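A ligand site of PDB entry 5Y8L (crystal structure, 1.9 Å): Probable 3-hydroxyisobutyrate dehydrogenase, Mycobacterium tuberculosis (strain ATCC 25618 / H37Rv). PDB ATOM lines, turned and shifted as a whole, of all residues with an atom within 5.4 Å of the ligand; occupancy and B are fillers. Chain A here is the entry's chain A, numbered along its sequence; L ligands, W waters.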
ATOM      1  N   LEU A   8     -30.975  -6.957 -17.166  1.00  0.00           N
ATOM      2  CA  LEU A   8     -30.269  -7.415 -15.992  1.00  0.00           C
ATOM      3  C   LEU A   8     -28.787  -7.214 -16.270  1.00  0.00           C
ATOM      4  O   LEU A   8     -28.183  -7.926 -17.094  1.00  0.00           O
ATOM      5  CB  LEU A   8     -30.611  -8.860 -15.763  1.00  0.00           C
ATOM      6  CG  LEU A   8     -32.092  -9.262 -15.799  1.00  0.00           C
ATOM      7  CD1 LEU A   8     -32.258 -10.782 -15.625  1.00  0.00           C
ATOM      8  CD2 LEU A   8     -32.824  -8.526 -14.706  1.00  0.00           C
ATOM      9  N   GLY A   9     -28.183  -6.268 -15.568  1.00  0.00           N
ATOM     10  CA  GLY A   9     -26.773  -5.878 -15.706  1.00  0.00           C
ATOM     11  C   GLY A   9     -26.753  -4.495 -16.353  1.00  0.00           C
ATOM     12  O   GLY A   9     -26.963  -4.374 -17.553  1.00  0.00           O
ATOM     13  N   LEU A  10     -26.600  -3.477 -15.519  1.00  0.00           N
ATOM     14  CA  LEU A  10     -26.723  -2.071 -15.937  1.00  0.00           C
ATOM     15  C   LEU A  10     -25.427  -1.351 -15.762  1.00  0.00           C
ATOM     16  O   LEU A  10     -25.361  -0.224 -15.258  1.00  0.00           O
ATOM     17  CB  LEU A  10     -27.844  -1.390 -15.104  1.00  0.00           C
ATOM     18  CG  LEU A  10     -29.260  -2.011 -15.302  1.00  0.00           C
ATOM     19  CD1 LEU A  10     -30.256  -1.552 -14.246  1.00  0.00           C
ATOM     20  CD2 LEU A  10     -29.842  -1.726 -16.628  1.00  0.00           C
ATOM     21  N   GLY A  11     -24.365  -2.025 -16.164  1.00  0.00           N
ATOM     22  CA  GLY A  11     -23.003  -1.563 -15.927  1.00  0.00           C
ATOM     23  C   GLY A  11     -22.518  -0.742 -17.107  1.00  0.00           C
ATOM     24  O   GLY A  11     -23.325  -0.020 -17.755  1.00  0.00           O
ATOM     25  N   ASN A  12     -21.232  -0.772 -17.380  1.00  0.00           N
ATOM     26  CA  ASN A  12     -20.665   0.037 -18.397  1.00  0.00           C
ATOM     27  C   ASN A  12     -21.341  -0.090 -19.766  1.00  0.00           C
ATOM     28  O   ASN A  12     -21.512   0.868 -20.444  1.00  0.00           O
ATOM     29  CB  ASN A  12     -19.166  -0.186 -18.474  1.00  0.00           C
ATOM     30  CG  ASN A  12     -18.446   0.390 -17.275  1.00  0.00           C
ATOM     31  OD1 ASN A  12     -18.752   1.460 -16.828  1.00  0.00           O
ATOM     32  ND2 ASN A  12     -17.523  -0.313 -16.767  1.00  0.00           N
ATOM     33  N   MET A  13     -21.649  -1.310 -20.141  1.00  0.00           N
ATOM     34  CA  MET A  13     -22.385  -1.572 -21.373  1.00  0.00           C
ATOM     35  C   MET A  13     -23.893  -1.533 -21.180  1.00  0.00           C
ATOM     36  O   MET A  13     -24.633  -0.892 -22.003  1.00  0.00           O
ATOM     37  CB  MET A  13     -21.960  -2.919 -21.928  1.00  0.00           C
ATOM     38  CG  MET A  13     -20.494  -3.006 -22.373  1.00  0.00           C
ATOM     39  SD  MET A  13     -20.094  -1.897 -23.753  1.00  0.00           S
ATOM     40  CE  MET A  13     -20.704  -2.793 -25.159  1.00  0.00           C
ATOM     41  N   GLY A  14     -24.393  -2.149 -20.107  1.00  0.00           N
ATOM     42  CA  GLY A  14     -25.841  -2.285 -19.914  1.00  0.00           C
ATOM     43  C   GLY A  14     -26.546  -0.933 -19.727  1.00  0.00           C
ATOM     44  O   GLY A  14     -27.699  -0.739 -20.167  1.00  0.00           O
ATOM     45  N   PHE A  31     -32.526  -4.419 -13.214  1.00  0.00           N
ATOM     46  CA  PHE A  31     -31.947  -4.854 -11.951  1.00  0.00           C
ATOM     47  C   PHE A  31     -30.448  -4.870 -12.071  1.00  0.00           C
ATOM     48  O   PHE A  31     -29.873  -5.308 -13.089  1.00  0.00           O
ATOM     49  CB  PHE A  31     -32.453  -6.213 -11.495  1.00  0.00           C
ATOM     50  CG  PHE A  31     -31.707  -6.730 -10.308  1.00  0.00           C
ATOM     51  CD1 PHE A  31     -31.929  -6.151  -9.069  1.00  0.00           C
ATOM     52  CD2 PHE A  31     -30.675  -7.665 -10.443  1.00  0.00           C
ATOM     53  CE1 PHE A  31     -31.225  -6.606  -7.957  1.00  0.00           C
ATOM     54  CE2 PHE A  31     -29.952  -8.088  -9.331  1.00  0.00           C
ATOM     55  CZ  PHE A  31     -30.256  -7.578  -8.099  1.00  0.00           C
ATOM     56  N   ASP A  32     -29.792  -4.385 -10.997  1.00  0.00           N
ATOM     57  CA  ASP A  32     -28.348  -4.433 -10.885  1.00  0.00           C
ATOM     58  C   ASP A  32     -28.045  -4.354  -9.381  1.00  0.00           C
ATOM     59  O   ASP A  32     -28.611  -3.553  -8.693  1.00  0.00           O
ATOM     60  CB  ASP A  32     -27.717  -3.305 -11.654  1.00  0.00           C
ATOM     61  CG  ASP A  32     -26.189  -3.463 -11.824  1.00  0.00           C
ATOM     62  OD1 ASP A  32     -25.476  -3.533 -10.796  1.00  0.00           O
ATOM     63  OD2 ASP A  32     -25.657  -3.553 -12.977  1.00  0.00           O
ATOM     64  N   PRO A  33     -27.193  -5.208  -8.871  1.00  0.00           N
ATOM     65  CA  PRO A  33     -26.896  -5.146  -7.415  1.00  0.00           C
ATOM     66  C   PRO A  33     -25.977  -4.011  -6.981  1.00  0.00           C
ATOM     67  O   PRO A  33     -25.775  -3.846  -5.771  1.00  0.00           O
ATOM     68  CB  PRO A  33     -26.249  -6.512  -7.150  1.00  0.00           C
ATOM     69  CG  PRO A  33     -25.630  -6.871  -8.488  1.00  0.00           C
ATOM     70  CD  PRO A  33     -26.554  -6.336  -9.521  1.00  0.00           C
ATOM     71  N   ALA A  34     -25.394  -3.251  -7.926  1.00  0.00           N
ATOM     72  CA  ALA A  34     -24.617  -2.065  -7.617  1.00  0.00           C
ATOM     73  C   ALA A  34     -25.537  -0.849  -7.656  1.00  0.00           C
ATOM     74  O   ALA A  34     -26.080  -0.524  -8.741  1.00  0.00           O
ATOM     75  CB  ALA A  34     -23.491  -1.915  -8.614  1.00  0.00           C
ATOM     76  N   ALA A  37     -24.978   1.817 -10.335  1.00  0.00           N
ATOM     77  CA  ALA A  37     -25.495   1.373 -11.656  1.00  0.00           C
ATOM     78  C   ALA A  37     -27.006   1.488 -11.771  1.00  0.00           C
ATOM     79  O   ALA A  37     -27.522   2.073 -12.724  1.00  0.00           O
ATOM     80  CB  ALA A  37     -25.069  -0.083 -11.940  1.00  0.00           C
ATOM     81  N   ALA A  52     -33.799  -9.539  -9.308  1.00  0.00           N
ATOM     82  CA  ALA A  52     -33.893  -9.925 -10.764  1.00  0.00           C
ATOM     83  C   ALA A  52     -35.247 -10.580 -11.115  1.00  0.00           C
ATOM     84  O   ALA A  52     -35.871 -10.232 -12.147  1.00  0.00           O
ATOM     85  CB  ALA A  52     -32.757 -10.785 -11.178  1.00  0.00           C
ATOM     86  N   MET A  65     -26.613  -8.582 -19.500  1.00  0.00           N
ATOM     87  CA  MET A  65     -25.337  -8.023 -19.887  1.00  0.00           C
ATOM     88  C   MET A  65     -24.426  -8.124 -18.674  1.00  0.00           C
ATOM     89  O   MET A  65     -24.219  -7.155 -17.939  1.00  0.00           O
ATOM     90  CB  MET A  65     -25.507  -6.548 -20.400  1.00  0.00           C
ATOM     91  CG  MET A  65     -24.291  -5.996 -21.123  1.00  0.00           C
ATOM     92  SD  MET A  65     -23.839  -7.050 -22.524  1.00  0.00           S
ATOM     93  CE  MET A  65     -22.574  -6.083 -23.386  1.00  0.00           C
ATOM     94  N   LEU A  66     -23.836  -9.287 -18.498  1.00  0.00           N
ATOM     95  CA  LEU A  66     -23.267  -9.673 -17.197  1.00  0.00           C
ATOM     96  C   LEU A  66     -21.814 -10.080 -17.332  1.00  0.00           C
ATOM     97  O   LEU A  66     -21.344 -10.211 -18.454  1.00  0.00           O
ATOM     98  CB  LEU A  66     -24.113 -10.771 -16.576  1.00  0.00           C
ATOM     99  CG  LEU A  66     -25.570 -10.484 -16.309  1.00  0.00           C
ATOM    100  CD1 LEU A  66     -26.267 -11.806 -15.941  1.00  0.00           C
ATOM    101  CD2 LEU A  66     -25.660  -9.483 -15.146  1.00  0.00           C
ATOM    102  N   PRO A  67     -21.080 -10.206 -16.212  1.00  0.00           N
ATOM    103  CA  PRO A  67     -19.605 -10.337 -16.389  1.00  0.00           C
ATOM    104  C   PRO A  67     -19.093 -11.667 -16.844  1.00  0.00           C
ATOM    105  O   PRO A  67     -18.109 -11.700 -17.543  1.00  0.00           O
ATOM    106  CB  PRO A  67     -19.011  -9.979 -15.010  1.00  0.00           C
ATOM    107  CG  PRO A  67     -20.105  -9.207 -14.305  1.00  0.00           C
ATOM    108  CD  PRO A  67     -21.422  -9.785 -14.844  1.00  0.00           C
ATOM    109  N   THR A  68     -19.748 -12.759 -16.474  1.00  0.00           N
ATOM    110  CA  THR A  68     -19.243 -14.086 -16.834  1.00  0.00           C
ATOM    111  C   THR A  68     -20.340 -15.127 -16.992  1.00  0.00           C
ATOM    112  O   THR A  68     -21.483 -14.889 -16.620  1.00  0.00           O
ATOM    113  CB  THR A  68     -18.371 -14.660 -15.713  1.00  0.00           C
ATOM    114  OG1 THR A  68     -19.182 -14.893 -14.588  1.00  0.00           O
ATOM    115  CG2 THR A  68     -17.190 -13.761 -15.367  1.00  0.00           C
ATOM    116  N   VAL A  71     -22.161 -16.143 -13.862  1.00  0.00           N
ATOM    117  CA  VAL A  71     -23.165 -15.187 -13.402  1.00  0.00           C
ATOM    118  C   VAL A  71     -24.399 -15.289 -14.292  1.00  0.00           C
ATOM    119  O   VAL A  71     -25.516 -15.250 -13.793  1.00  0.00           O
ATOM    120  CB  VAL A  71     -22.583 -13.743 -13.336  1.00  0.00           C
ATOM    121  CG1 VAL A  71     -23.646 -12.710 -12.999  1.00  0.00           C
ATOM    122  CG2 VAL A  71     -21.457 -13.671 -12.325  1.00  0.00           C
ATOM    123  N   CYS A  75     -28.074 -16.291 -12.880  1.00  0.00           N
ATOM    124  CA  CYS A  75     -29.164 -15.340 -13.155  1.00  0.00           C
ATOM    125  C   CYS A  75     -30.345 -16.092 -13.832  1.00  0.00           C
ATOM    126  O   CYS A  75     -31.480 -15.956 -13.437  1.00  0.00           O
ATOM    127  CB  CYS A  75     -28.631 -14.222 -14.052  1.00  0.00           C
ATOM    128  SG  CYS A  75     -29.919 -13.049 -14.572  1.00  0.00           S
ATOM    129  N   SER A  92     -26.346 -10.930 -24.121  1.00  0.00           N
ATOM    130  CA  SER A  92     -25.358 -10.146 -24.796  1.00  0.00           C
ATOM    131  C   SER A  92     -24.038 -10.103 -24.031  1.00  0.00           C
ATOM    132  O   SER A  92     -23.111  -9.436 -24.451  1.00  0.00           O
ATOM    133  CB  SER A  92     -25.937  -8.768 -25.074  1.00  0.00           C
ATOM    134  OG  SER A  92     -26.859  -8.887 -26.172  1.00  0.00           O
ATOM    135  N   SER A  93     -23.959 -10.791 -22.910  1.00  0.00           N
ATOM    136  CA  SER A  93     -22.652 -11.032 -22.263  1.00  0.00           C
ATOM    137  C   SER A  93     -21.659 -11.723 -23.225  1.00  0.00           C
ATOM    138  O   SER A  93     -22.054 -12.439 -24.158  1.00  0.00           O
ATOM    139  CB  SER A  93     -22.813 -11.862 -20.981  1.00  0.00           C
ATOM    140  OG  SER A  93     -23.960 -11.407 -20.303  1.00  0.00           O
ATOM    141  N   THR A  94     -20.373 -11.579 -22.908  1.00  0.00           N
ATOM    142  CA  THR A  94     -19.340 -12.308 -23.612  1.00  0.00           C
ATOM    143  C   THR A  94     -18.961 -13.491 -22.698  1.00  0.00           C
ATOM    144  O   THR A  94     -18.417 -13.297 -21.665  1.00  0.00           O
ATOM    145  CB  THR A  94     -18.098 -11.481 -23.945  1.00  0.00           C
ATOM    146  OG1 THR A  94     -18.483 -10.339 -24.667  1.00  0.00           O
ATOM    147  CG2 THR A  94     -17.136 -12.284 -24.766  1.00  0.00           C
ATOM    148  N   ILE A  95     -19.396 -14.675 -23.071  1.00  0.00           N
ATOM    149  CA  ILE A  95     -19.157 -15.889 -22.305  1.00  0.00           C
ATOM    150  C   ILE A  95     -18.733 -17.063 -23.225  1.00  0.00           C
ATOM    151  O   ILE A  95     -18.849 -16.975 -24.388  1.00  0.00           O
ATOM    152  CB  ILE A  95     -20.377 -16.306 -21.464  1.00  0.00           C
ATOM    153  CG1 ILE A  95     -21.525 -16.828 -22.335  1.00  0.00           C
ATOM    154  CG2 ILE A  95     -20.843 -15.214 -20.508  1.00  0.00           C
ATOM    155  CD1 ILE A  95     -22.758 -17.211 -21.557  1.00  0.00           C
ATOM    156  N   VAL A 119     -21.608  -8.625 -28.205  1.00  0.00           N
ATOM    157  CA  VAL A 119     -21.329  -7.429 -28.971  1.00  0.00           C
ATOM    158  C   VAL A 119     -19.910  -7.008 -29.063  1.00  0.00           C
ATOM    159  O   VAL A 119     -19.071  -7.319 -28.196  1.00  0.00           O
ATOM    160  CB  VAL A 119     -22.141  -6.227 -28.446  1.00  0.00           C
ATOM    161  CG1 VAL A 119     -23.655  -6.553 -28.449  1.00  0.00           C
ATOM    162  CG2 VAL A 119     -21.681  -5.787 -27.068  1.00  0.00           C
ATOM    163  N   SER A 120     -19.632  -6.254 -30.139  1.00  0.00           N
ATOM    164  CA  SER A 120     -18.394  -5.477 -30.309  1.00  0.00           C
ATOM    165  C   SER A 120     -18.721  -3.992 -30.443  1.00  0.00           C
ATOM    166  O   SER A 120     -19.748  -3.660 -31.045  1.00  0.00           O
ATOM    167  CB  SER A 120     -17.730  -5.937 -31.589  1.00  0.00           C
ATOM    168  OG  SER A 120     -17.392  -7.300 -31.452  1.00  0.00           O
ATOM    169  N   GLY A 121     -17.849  -3.131 -29.921  1.00  0.00           N
ATOM    170  CA  GLY A 121     -17.952  -1.694 -30.096  1.00  0.00           C
ATOM    171  C   GLY A 121     -17.740  -0.870 -28.818  1.00  0.00           C
ATOM    172  O   GLY A 121     -17.700   0.368 -28.882  1.00  0.00           O
ATOM    173  N   GLY A 122     -17.631  -1.489 -27.662  1.00  0.00           N
ATOM    174  CA  GLY A 122     -17.367  -0.733 -26.445  1.00  0.00           C
ATOM    175  C   GLY A 122     -18.461   0.187 -25.967  1.00  0.00           C
ATOM    176  O   GLY A 122     -19.591   0.228 -26.518  1.00  0.00           O
ATOM    177  N   VAL A 123     -18.145   0.896 -24.910  1.00  0.00           N
ATOM    178  CA  VAL A 123     -19.031   1.894 -24.320  1.00  0.00           C
ATOM    179  C   VAL A 123     -19.428   2.999 -25.342  1.00  0.00           C
ATOM    180  O   VAL A 123     -20.565   3.427 -25.390  1.00  0.00           O
ATOM    181  CB  VAL A 123     -18.420   2.444 -23.038  1.00  0.00           C
ATOM    182  CG1 VAL A 123     -19.164   3.654 -22.489  1.00  0.00           C
ATOM    183  CG2 VAL A 123     -18.442   1.350 -22.005  1.00  0.00           C
ATOM    184  N   LYS A 169     -17.464 -14.232 -32.312  1.00  0.00           N
ATOM    185  CA  LYS A 169     -16.752 -13.147 -31.656  1.00  0.00           C
ATOM    186  C   LYS A 169     -15.395 -13.633 -31.098  1.00  0.00           C
ATOM    187  O   LYS A 169     -14.428 -12.934 -31.203  1.00  0.00           O
ATOM    188  CB  LYS A 169     -17.495 -12.565 -30.518  1.00  0.00           C
ATOM    189  CG  LYS A 169     -16.761 -11.444 -29.813  1.00  0.00           C
ATOM    190  CD  LYS A 169     -17.570 -10.727 -28.725  1.00  0.00           C
ATOM    191  CE  LYS A 169     -16.670  -9.711 -28.019  1.00  0.00           C
ATOM    192  NZ  LYS A 169     -17.411  -9.028 -26.975  1.00  0.00           N
ATOM    193  N   LEU A 241      -9.969  -6.146 -21.330  1.00  0.00           N
ATOM    194  CA  LEU A 241     -11.011  -6.817 -22.132  1.00  0.00           C
ATOM    195  C   LEU A 241     -10.446  -7.793 -23.169  1.00  0.00           C
ATOM    196  O   LEU A 241     -10.978  -8.845 -23.376  1.00  0.00           O
ATOM    197  CB  LEU A 241     -11.915  -5.797 -22.802  1.00  0.00           C
ATOM    198  CG  LEU A 241     -13.017  -5.224 -21.894  1.00  0.00           C
ATOM    199  CD1 LEU A 241     -13.611  -3.959 -22.516  1.00  0.00           C
ATOM    200  CD2 LEU A 241     -14.095  -6.329 -21.729  1.00  0.00           C
ATOM    201  N   LYS A 244      -9.517 -10.828 -21.287  1.00  0.00           N
ATOM    202  CA  LYS A 244     -10.750 -11.577 -21.041  1.00  0.00           C
ATOM    203  C   LYS A 244     -11.184 -12.424 -22.249  1.00  0.00           C
ATOM    204  O   LYS A 244     -11.443 -13.598 -22.122  1.00  0.00           O
ATOM    205  CB  LYS A 244     -11.875 -10.618 -20.626  1.00  0.00           C
ATOM    206  CG  LYS A 244     -13.260 -11.302 -20.625  1.00  0.00           C
ATOM    207  CD  LYS A 244     -14.367 -10.439 -20.003  1.00  0.00           C
ATOM    208  CE  LYS A 244     -15.519 -11.204 -19.376  1.00  0.00           C
ATOM    209  NZ  LYS A 244     -16.607 -11.421 -20.366  1.00  0.00           N
ATOM    210  N   ASP A 245     -11.261 -11.814 -23.431  1.00  0.00           N
ATOM    211  CA  ASP A 245     -11.655 -12.523 -24.618  1.00  0.00           C
ATOM    212  C   ASP A 245     -10.718 -13.649 -25.030  1.00  0.00           C
ATOM    213  O   ASP A 245     -11.136 -14.736 -25.497  1.00  0.00           O
ATOM    214  CB  ASP A 245     -11.827 -11.518 -25.775  1.00  0.00           C
ATOM    215  CG  ASP A 245     -13.071 -10.656 -25.632  1.00  0.00           C
ATOM    216  OD1 ASP A 245     -14.001 -11.025 -24.798  1.00  0.00           O
ATOM    217  OD2 ASP A 245     -13.130  -9.590 -26.363  1.00  0.00           O
HETATM  218  P1  LIG L   1     -19.696  -4.119 -15.890  1.00  0.00           P
HETATM  219  O1  LIG L   1     -19.060  -4.802 -14.811  1.00  0.00           O
HETATM  220  O2  LIG L   1     -19.520  -2.748 -15.985  1.00  0.00           O
HETATM  221  O3  LIG L   1     -21.226  -4.382 -15.785  1.00  0.00           O
HETATM  222  C1  LIG L   1     -21.796  -5.586 -15.315  1.00  0.00           C
HETATM  223  C2  LIG L   1     -22.899  -5.346 -14.298  1.00  0.00           C
HETATM  224  O4  LIG L   1     -23.598  -6.495 -13.950  1.00  0.00           O
HETATM  225  C3  LIG L   1     -22.398  -4.739 -12.987  1.00  0.00           C
HETATM  226  O5  LIG L   1     -22.965  -3.451 -12.837  1.00  0.00           O
HETATM  227  C4  LIG L   1     -22.834  -5.735 -11.925  1.00  0.00           C
HETATM  228  O6  LIG L   1     -23.193  -5.122 -10.742  1.00  0.00           O
HETATM  229  C5  LIG L   1     -24.018  -6.394 -12.628  1.00  0.00           C
HETATM  230  N1  LIG L   1     -24.483  -7.710 -12.149  1.00  0.00           N
HETATM  231  C6  LIG L   1     -23.803  -8.718 -11.620  1.00  0.00           C
HETATM  232  N2  LIG L   1     -24.603  -9.748 -11.348  1.00  0.00           N
HETATM  233  C7  LIG L   1     -25.817  -9.409 -11.700  1.00  0.00           C
HETATM  234  C8  LIG L   1     -27.135 -10.030 -11.720  1.00  0.00           C
HETATM  235  N3  LIG L   1     -27.309 -11.268 -11.257  1.00  0.00           N
HETATM  236  N4  LIG L   1     -28.149  -9.294 -12.178  1.00  0.00           N
HETATM  237  C9  LIG L   1     -27.968  -8.073 -12.648  1.00  0.00           C
HETATM  238  N5  LIG L   1     -26.814  -7.478 -12.705  1.00  0.00           N
HETATM  239  C10 LIG L   1     -25.736  -8.068 -12.245  1.00  0.00           C
HETATM  240  O7  LIG L   1     -19.200  -4.798 -17.214  1.00  0.00           O
HETATM  241  P2  LIG L   1     -19.545  -4.361 -18.673  1.00  0.00           P
HETATM  242  O8  LIG L   1     -18.470  -3.666 -19.220  1.00  0.00           O
HETATM  243  O9  LIG L   1     -20.831  -3.755 -18.739  1.00  0.00           O
HETATM  244  O10 LIG L   1     -19.572  -5.717 -19.446  1.00  0.00           O
HETATM  245  C11 LIG L   1     -20.590  -6.659 -19.427  1.00  0.00           C
HETATM  246  C12 LIG L   1     -20.398  -7.733 -20.486  1.00  0.00           C
HETATM  247  O11 LIG L   1     -20.171  -7.111 -21.713  1.00  0.00           O
HETATM  248  C13 LIG L   1     -19.166  -8.597 -20.263  1.00  0.00           C
HETATM  249  O12 LIG L   1     -19.447  -9.926 -20.554  1.00  0.00           O
HETATM  250  C14 LIG L   1     -18.127  -7.999 -21.186  1.00  0.00           C
HETATM  251  O13 LIG L   1     -17.191  -8.907 -21.691  1.00  0.00           O
HETATM  252  C15 LIG L   1     -18.987  -7.496 -22.324  1.00  0.00           C
HETATM  253  N6  LIG L   1     -18.438  -6.450 -23.176  1.00  0.00           N
HETATM  254  C16 LIG L   1     -17.913  -5.364 -22.679  1.00  0.00           C
HETATM  255  C17 LIG L   1     -17.427  -4.343 -23.484  1.00  0.00           C
HETATM  256  C18 LIG L   1     -16.849  -3.107 -22.874  1.00  0.00           C
HETATM  257  O14 LIG L   1     -16.283  -2.350 -23.563  1.00  0.00           O
HETATM  258  N7  LIG L   1     -16.968  -2.883 -21.586  1.00  0.00           N
HETATM  259  C19 LIG L   1     -17.500  -4.530 -24.860  1.00  0.00           C
HETATM  260  C20 LIG L   1     -18.048  -5.690 -25.346  1.00  0.00           C
HETATM  261  C21 LIG L   1     -18.534  -6.625 -24.469  1.00  0.00           C
HETATM  262  O   HOH W   1     -21.390  -1.561 -11.913  1.00  0.00           O
HETATM  263  O   HOH W   2     -23.593  -4.167 -18.012  1.00  0.00           O
HETATM  264  O   HOH W   3     -14.363  -2.337 -25.453  1.00  0.00           O
HETATM  265  O   HOH W   4     -16.403  -3.898 -14.413  1.00  0.00           O
HETATM  266  O   HOH W   5     -19.306  -6.333 -12.408  1.00  0.00           O
HETATM  267  O   HOH W   6     -17.682  -7.272 -16.644  1.00  0.00           O
HETATM  268  O   HOH W   7     -26.243 -14.189 -11.168  1.00  0.00           O
HETATM  269  O   HOH W   8     -15.440   0.172 -23.725  1.00  0.00           O
HETATM  270  O   HOH W   9     -19.591  -1.104 -13.805  1.00  0.00           O
HETATM  271  O   HOH W  10     -15.684  -0.384 -20.221  1.00  0.00           O
HETATM  272  O   HOH W  11     -24.210 -11.772  -9.749  1.00  0.00           O
HETATM  273  O   HOH W  12     -16.606  -2.297 -18.242  1.00  0.00           O
HETATM  274  O   HOH W  13     -20.794  -4.884  -9.874  1.00  0.00           O
HETATM  275  O   HOH W  14     -15.819  -7.624 -18.779  1.00  0.00           O
HETATM  276  O   HOH W  15     -15.418  -4.491 -18.100  1.00  0.00           O
HETATM  277  O   HOH W  16     -15.790  -9.113 -23.895  1.00  0.00           O
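SD of Met 65 lies close to O11 of the ligand (3.8 Å).
C of Leu 8 touches C9 of the ligand, 3.8 Å away.
Gly 11 touches the ligand.
O of Phe 31 touches C9 of the ligand, 3.4 Å away.
Pro 33 touches the ligand.
Ala 34 touches the ligand (CB to O6, 3.9 Å).
O of Pro 67 touches O12 of the ligand, at 3.7 Å.
CG1 of Val 71 touches N2 of the ligand, at 3.5 Å.
CA of Ser 93 touches O12 of the ligand, at 3.8 Å.
Val 119 touches the ligand (O to C20, 3.4 Å).
CA of Gly 122 touches O14 of the ligand, at 3.5 Å.
Val 123 touches the ligand.
Lys 169 touches the ligand.
CD1 of Leu 241 touches O14 of the ligand, 3.3 Å away.
Hydrophobic or aromatic side chains within 4 Å of the ligand: Met 13, Phe 31, Pro 33, Ala 34, Met 65, Leu 66, Val 71 and Leu 241.
Of the 32 residues printed, 21 come within 4 Å of the ligand.
Along chain A the residues within 4 Å of the ligand span positions 8 to 244.
The nearest printed residue that does not touch the ligand is Ala 37 (4.1 Å).
The backbone NH of Leu 10 sits at hydrogen-bond distance from the side-chain carboxylate of Asp 32 (2.7 Å).
NZ of Lys 244 sits at hydrogen-bond distance from O of Thr 94, at 2.9 Å.
SD of Met 65 lies within hydrogen-bond range of N of Ser 93 (3.8 Å).
The backbone NH of Val 71 lies within hydrogen-bond range of the side-chain hydroxyl of Thr 68, 3.3 Å away.
NZ of Lys 169 is in hydrogen-bond range of OG1 of Thr 94 (2.9 Å).
The side-chain amino group (NZ) of Lys 244 sits at hydrogen-bond distance from the backbone carbonyl oxygen (O) of Pro 67 (3.2 Å).
NZ of Lys 169 lies within hydrogen-bond range of O of Val 119.
SD of Met 13 lies within hydrogen-bond range of N of Val 123, 3.6 Å away.
Water W12 bridges an oxygen (O8) of the ligand (2.5 Å) and the side-chain amide nitrogen of Asn 12 (2.6 Å).
Water W16 lies within hydrogen-bond range of an oxygen (O13) of the ligand, the side-chain carboxylate (OD1) of Asp 245, the side-chain hydroxyl (OG1) of Thr 94 and the side-chain amino group (NZ) of Lys 169.
Water W8 lies within hydrogen-bond range of an oxygen (O14) of the ligand and the backbone NH (N) of Val 123.
Water W2 lies within hydrogen-bond range of O9 of the ligand (2.9 Å), N of Gly 11 (2.9 Å), N of Gly 14 (3.0 Å), O of Met 65 (3.1 Å) and O of Gly 9 (3.4 Å).
Water W7 lies within hydrogen-bond range of O of Val 71, N3 of the ligand and N of Cys 75.
The backbone NH (N) of Asn 12 is in hydrogen-bond range of an oxygen (O2) of the ligand (3.0 Å).
An oxygen (O9) of the ligand is in hydrogen-bond range of the backbone NH (N) of Met 13 (2.9 Å).
OD2 of Asp 32 is in hydrogen-bond range of O5 of the ligand.
The side-chain amino group (NZ) of Lys 244 lies within hydrogen-bond range of an oxygen (O13) of the ligand (2.9 Å).
The backbone NH (N) of Gly 9 sits at hydrogen-bond distance from a nitrogen (N5) of the ligand.
O12 of the ligand sits at hydrogen-bond distance from N of Thr 94 (3.0 Å).
ND2 of Asn 12 lies within hydrogen-bond range of O2 of the ligand (3.2 Å).
O of Leu 66 lies within hydrogen-bond range of O12 of the ligand.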
